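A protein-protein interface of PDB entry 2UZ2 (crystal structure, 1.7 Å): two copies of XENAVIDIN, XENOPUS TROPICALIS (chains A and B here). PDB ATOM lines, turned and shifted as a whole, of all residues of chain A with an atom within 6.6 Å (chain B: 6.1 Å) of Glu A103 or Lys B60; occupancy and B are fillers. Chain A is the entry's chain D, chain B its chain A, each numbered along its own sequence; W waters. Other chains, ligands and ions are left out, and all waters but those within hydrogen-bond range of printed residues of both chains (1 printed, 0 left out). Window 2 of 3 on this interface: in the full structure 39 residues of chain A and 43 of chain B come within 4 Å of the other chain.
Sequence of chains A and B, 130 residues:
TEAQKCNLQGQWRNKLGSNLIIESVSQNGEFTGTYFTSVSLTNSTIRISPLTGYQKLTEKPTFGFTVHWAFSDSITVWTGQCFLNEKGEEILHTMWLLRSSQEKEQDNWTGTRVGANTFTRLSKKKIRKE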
ATOM      1  N   SER A 101      -4.617  -2.273   6.022  1.00  0.00           N
ATOM      2  CA  SER A 101      -4.146  -1.901   7.326  1.00  0.00           C
ATOM      3  C   SER A 101      -5.107  -0.950   8.049  1.00  0.00           C
ATOM      4  O   SER A 101      -5.339   0.194   7.623  1.00  0.00           O
ATOM      5  CB  SER A 101      -2.743  -1.303   7.194  1.00  0.00           C
ATOM      6  OG  SER A 101      -2.320  -0.832   8.443  1.00  0.00           O
ATOM      7  N   GLN A 102      -5.673  -1.453   9.145  1.00  0.00           N
ATOM      8  CA  GLN A 102      -6.551  -0.701  10.009  1.00  0.00           C
ATOM      9  C   GLN A 102      -5.809  -0.010  11.154  1.00  0.00           C
ATOM     10  O   GLN A 102      -4.741  -0.474  11.602  1.00  0.00           O
ATOM     11  CB  GLN A 102      -7.664  -1.600  10.549  1.00  0.00           C
ATOM     12  CG  GLN A 102      -8.525  -2.245   9.447  1.00  0.00           C
ATOM     13  CD  GLN A 102      -9.027  -1.226   8.446  1.00  0.00           C
ATOM     14  OE1 GLN A 102      -9.587  -0.199   8.819  1.00  0.00           O
ATOM     15  NE2 GLN A 102      -8.738  -1.464   7.182  1.00  0.00           N
ATOM     16  N   GLU A 103      -6.385   1.100  11.618  1.00  0.00           N
ATOM     17  CA  GLU A 103      -5.732   1.966  12.613  1.00  0.00           C
ATOM     18  C   GLU A 103      -5.773   1.345  14.004  1.00  0.00           C
ATOM     19  O   GLU A 103      -4.869   1.544  14.817  1.00  0.00           O
ATOM     20  CB  GLU A 103      -6.394   3.355  12.650  1.00  0.00           C
ATOM     21  CG  GLU A 103      -6.338   4.118  11.322  1.00  0.00           C
ATOM     22  CD  GLU A 103      -6.874   5.529  11.420  1.00  0.00           C
ATOM     23  OE1 GLU A 103      -8.037   5.733  11.879  1.00  0.00           O
ATOM     24  OE2 GLU A 103      -6.119   6.459  11.048  1.00  0.00           O
ATOM     25  N   LYS A 104      -6.858   0.639  14.302  1.00  0.00           N
ATOM     26  CA  LYS A 104      -7.061   0.097  15.637  1.00  0.00           C
ATOM     27  C   LYS A 104      -7.798  -1.211  15.574  1.00  0.00           C
ATOM     28  O   LYS A 104      -8.502  -1.493  14.602  1.00  0.00           O
ATOM     29  CB  LYS A 104      -7.825   1.069  16.526  1.00  0.00           C
ATOM     30  CG  LYS A 104      -9.111   1.590  15.951  1.00  0.00           C
ATOM     31  CD  LYS A 104      -9.587   2.808  16.759  1.00  0.00           C
ATOM     32  CE  LYS A 104     -10.687   3.577  16.034  1.00  0.00           C
ATOM     33  NZ  LYS A 104     -10.225   4.034  14.682  1.00  0.00           N
ATOM     34  N   GLU A 105      -7.645  -1.996  16.635  1.00  0.00           N
ATOM     35  CA  GLU A 105      -8.250  -3.309  16.727  1.00  0.00           C
ATOM     36  C   GLU A 105      -9.756  -3.283  16.511  1.00  0.00           C
ATOM     37  O   GLU A 105     -10.289  -4.176  15.844  1.00  0.00           O
ATOM     38  CB  GLU A 105      -7.944  -3.952  18.073  1.00  0.00           C
ATOM     39  CG  GLU A 105      -8.210  -5.441  18.041  1.00  0.00           C
ATOM     40  CD  GLU A 105      -8.248  -6.067  19.403  1.00  0.00           C
ATOM     41  OE1 GLU A 105      -8.166  -5.328  20.406  1.00  0.00           O
ATOM     42  OE2 GLU A 105      -8.369  -7.309  19.469  1.00  0.00           O
ATOM     43  N   ASP A 107     -11.486  -1.708  14.552  1.00  0.00           N
ATOM     44  CA  ASP A 107     -11.857  -1.556  13.140  1.00  0.00           C
ATOM     45  C   ASP A 107     -11.476  -2.795  12.350  1.00  0.00           C
ATOM     46  O   ASP A 107     -11.549  -2.811  11.114  1.00  0.00           O
ATOM     47  CB  ASP A 107     -11.154  -0.351  12.490  1.00  0.00           C
ATOM     48  CG  ASP A 107     -11.587   0.987  13.068  1.00  0.00           C
ATOM     49  OD1 ASP A 107     -12.706   1.131  13.579  1.00  0.00           O
ATOM     50  OD2 ASP A 107     -10.785   1.928  12.988  1.00  0.00           O
ATOM     51  N   LYS B   5       5.668  -5.376  19.602  1.00  0.00           N
ATOM     52  CA  LYS B   5       5.361  -4.460  18.508  1.00  0.00           C
ATOM     53  C   LYS B   5       5.062  -5.258  17.250  1.00  0.00           C
ATOM     54  O   LYS B   5       5.387  -4.823  16.136  1.00  0.00           O
ATOM     55  CB  LYS B   5       6.523  -3.486  18.245  1.00  0.00           C
ATOM     56  CG  LYS B   5       6.654  -2.317  19.238  1.00  0.00           C
ATOM     57  CD  LYS B   5       5.297  -1.718  19.672  1.00  0.00           C
ATOM     58  CE  LYS B   5       4.711  -0.712  18.680  1.00  0.00           C
ATOM     59  NZ  LYS B   5       5.308   0.654  18.798  1.00  0.00           N
ATOM     60  N   CYS B   6       4.471  -6.439  17.445  1.00  0.00           N
ATOM     61  CA  CYS B   6       3.983  -7.285  16.363  1.00  0.00           C
ATOM     62  C   CYS B   6       5.028  -7.811  15.377  1.00  0.00           C
ATOM     63  O   CYS B   6       4.763  -7.964  14.174  1.00  0.00           O
ATOM     64  CB  CYS B   6       2.837  -6.597  15.637  1.00  0.00           C
ATOM     65  SG  CYS B   6       1.396  -6.279  16.700  1.00  0.00           S
ATOM     66  N   THR B  58       5.546  -2.176   9.593  1.00  0.00           N
ATOM     67  CA  THR B  58       4.887  -1.056  10.271  1.00  0.00           C
ATOM     68  C   THR B  58       4.394  -1.462  11.650  1.00  0.00           C
ATOM     69  O   THR B  58       4.350  -2.648  11.987  1.00  0.00           O
ATOM     70  CB  THR B  58       3.625  -0.659   9.494  1.00  0.00           C
ATOM     71  OG1 THR B  58       2.883  -1.841   9.217  1.00  0.00           O
ATOM     72  CG2 THR B  58       3.973   0.010   8.196  1.00  0.00           C
ATOM     73  N   GLU B  59       3.974  -0.469  12.436  1.00  0.00           N
ATOM     74  CA  GLU B  59       3.212  -0.771  13.620  1.00  0.00           C
ATOM     75  C   GLU B  59       1.874  -1.406  13.206  1.00  0.00           C
ATOM     76  O   GLU B  59       1.138  -0.902  12.292  1.00  0.00           O
ATOM     77  CB  GLU B  59       2.943   0.483  14.473  1.00  0.00           C
ATOM     78  CG  GLU B  59       2.709   0.206  15.966  1.00  0.00           C
ATOM     79  CD  GLU B  59       1.997   1.352  16.708  1.00  0.00           C
ATOM     80  OE1 GLU B  59       1.781   2.452  16.122  1.00  0.00           O
ATOM     81  OE2 GLU B  59       1.685   1.161  17.913  1.00  0.00           O
ATOM     82  N   LYS B  60       1.538  -2.458  13.951  1.00  0.00           N
ATOM     83  CA  LYS B  60       0.326  -3.248  13.776  1.00  0.00           C
ATOM     84  C   LYS B  60       0.336  -3.824  12.362  1.00  0.00           C
ATOM     85  O   LYS B  60      -0.522  -3.484  11.529  1.00  0.00           O
ATOM     86  CB  LYS B  60      -0.941  -2.430  14.028  1.00  0.00           C
ATOM     87  CG  LYS B  60      -1.031  -1.828  15.427  1.00  0.00           C
ATOM     88  CD  LYS B  60      -2.137  -0.800  15.497  1.00  0.00           C
ATOM     89  CE  LYS B  60      -1.686   0.488  14.816  1.00  0.00           C
ATOM     90  NZ  LYS B  60      -2.057   1.688  15.594  1.00  0.00           N
ATOM     91  N   PRO B  61       1.339  -4.648  12.089  1.00  0.00           N
ATOM     92  CA  PRO B  61       1.555  -5.072  10.719  1.00  0.00           C
ATOM     93  C   PRO B  61       0.460  -5.987  10.195  1.00  0.00           C
ATOM     94  O   PRO B  61       0.010  -6.900  10.894  1.00  0.00           O
ATOM     95  CB  PRO B  61       2.862  -5.819  10.787  1.00  0.00           C
ATOM     96  CG  PRO B  61       3.013  -6.258  12.202  1.00  0.00           C
ATOM     97  CD  PRO B  61       2.354  -5.195  13.009  1.00  0.00           C
ATOM     98  N   THR B  62       0.096  -5.752   8.944  1.00  0.00           N
ATOM     99  CA  THR B  62      -0.607  -6.765   8.164  1.00  0.00           C
ATOM    100  C   THR B  62       0.362  -7.853   7.723  1.00  0.00           C
ATOM    101  O   THR B  62       1.605  -7.691   7.767  1.00  0.00           O
ATOM    102  CB  THR B  62      -1.240  -6.144   6.923  1.00  0.00           C
ATOM    103  OG1 THR B  62      -0.229  -5.411   6.200  1.00  0.00           O
ATOM    104  CG2 THR B  62      -2.381  -5.148   7.362  1.00  0.00           C
ATOM    105  N   GLN B  81      -3.966  -9.063  10.517  1.00  0.00           N
ATOM    106  CA  GLN B  81      -3.251  -7.936  11.064  1.00  0.00           C
ATOM    107  C   GLN B  81      -3.020  -8.214  12.535  1.00  0.00           C
ATOM    108  O   GLN B  81      -3.894  -8.767  13.212  1.00  0.00           O
ATOM    109  CB  GLN B  81      -4.026  -6.630  10.846  1.00  0.00           C
ATOM    110  CG  GLN B  81      -3.275  -5.336  11.280  1.00  0.00           C
ATOM    111  CD  GLN B  81      -3.927  -4.055  10.836  1.00  0.00           C
ATOM    112  OE1 GLN B  81      -5.048  -4.051  10.280  1.00  0.00           O
ATOM    113  NE2 GLN B  81      -3.277  -2.919  11.162  1.00  0.00           N
ATOM    114  N   CYS B  82      -1.854  -7.799  13.028  1.00  0.00           N
ATOM    115  CA  CYS B  82      -1.518  -7.945  14.428  1.00  0.00           C
ATOM    116  C   CYS B  82      -1.855  -6.667  15.188  1.00  0.00           C
ATOM    117  O   CYS B  82      -1.516  -5.580  14.729  1.00  0.00           O
ATOM    118  CB  CYS B  82      -0.020  -8.202  14.545  1.00  0.00           C
ATOM    119  SG  CYS B  82       0.531  -8.565  16.208  1.00  0.00           S
ATOM    120  N   PHE B  83      -2.535  -6.807  16.332  1.00  0.00           N
ATOM    121  CA  PHE B  83      -2.841  -5.692  17.231  1.00  0.00           C
ATOM    122  C   PHE B  83      -2.437  -6.076  18.652  1.00  0.00           C
ATOM    123  O   PHE B  83      -2.254  -7.263  18.956  1.00  0.00           O
ATOM    124  CB  PHE B  83      -4.344  -5.394  17.224  1.00  0.00           C
ATOM    125  CG  PHE B  83      -4.887  -4.958  15.889  1.00  0.00           C
ATOM    126  CD1 PHE B  83      -4.813  -3.621  15.495  1.00  0.00           C
ATOM    127  CD2 PHE B  83      -5.520  -5.863  15.060  1.00  0.00           C
ATOM    128  CE1 PHE B  83      -5.355  -3.214  14.253  1.00  0.00           C
ATOM    129  CE2 PHE B  83      -6.053  -5.472  13.817  1.00  0.00           C
ATOM    130  CZ  PHE B  83      -5.981  -4.134  13.436  1.00  0.00           C
ATOM    131  N   LEU B  84      -2.290  -5.075  19.510  1.00  0.00           N
ATOM    132  CA  LEU B  84      -2.170  -5.311  20.946  1.00  0.00           C
ATOM    133  C   LEU B  84      -3.573  -5.217  21.504  1.00  0.00           C
ATOM    134  O   LEU B  84      -4.246  -4.203  21.304  1.00  0.00           O
ATOM    135  CB  LEU B  84      -1.254  -4.271  21.615  1.00  0.00           C
ATOM    136  CG  LEU B  84       0.166  -4.065  21.061  1.00  0.00           C
ATOM    137  CD1 LEU B  84       0.918  -3.016  21.857  1.00  0.00           C
ATOM    138  CD2 LEU B  84       0.970  -5.362  21.033  1.00  0.00           C
HETATM  139  O   HOH W   1       0.029  -2.416   9.379  1.00  0.00           O
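No position is printed for both chains. Of the 7 pairs that touch across the chains among the printed residues, none has its exchanged pair printed and touching as well.
Ser A101 touches Thr B62. Gln B81 touches Ser A101. Gln A102 touches Phe B83. Phe B83 touches Lys A104 (CE1 to C, 3.4 Å). Glu A105 touches Phe B83 (N to CD1, 3.5 Å).
The side-chain carboxylate of Glu B59 is in salt-bridge range of the side-chain amino group of Lys B60. The side-chain amide nitrogen (NE2) of Gln B81 is in hydrogen-bond range of the backbone carbonyl oxygen (O) of Lys B60 (2.8 Å). The side-chain carboxylate (OE1) of Glu A103 lies within salt-bridge range of the side-chain amino group (NZ) of Lys A104 (3.9 Å). The side-chain amino group (NZ) of Lys A104 is in salt-bridge range of the side-chain carboxylate (OD2) of Asp A107 (2.8 Å). SG of Cys B6 forms a disulfide with SG of Cys B82, at 2.5 Å.
The side-chain amino group (NZ) of Lys B60 sits at hydrogen-bond distance from the backbone carbonyl oxygen (O) of Glu A103, at 2.9 Å. O of Gln A102 lies within hydrogen-bond range of NE2 of Gln B81 (2.9 Å).
Glu A103 touches just one residue of chain B: Lys B60 (2.9 Å). Lys B60 touches just one residue of chain A: Glu A103. Of the printed residues of chain B, Glu A105 touches Phe B83. Printed residues of chain B within 4 Å of Gln A102: Gln B81 (2.9 Å) and Phe B83 (3.9 Å). The nearest residue of chain B that does not touch Glu A103 is Phe B83 (4.6 Å).
Water W1 lies within hydrogen-bond range of O of Lys B60 (2.5 Å), OG1 of Thr B58 (2.9 Å), OG of Ser A101 (3.0 Å), N of Thr B62 (3.4 Å) and O of Glu B59 (3.5 Å).
Hydrophobic or aromatic side chains of chain B that line the printed part of chain A: Phe B83. Of the 6 printed residues of chain A, 5 touch a printed residue of chain B. Printed residues of chain A that touch a printed residue of chain B: Ser A101, Gln A102, Glu A103, Lys A104 and Glu A105. Among the printed residues, 7 pairs touch across the chains.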
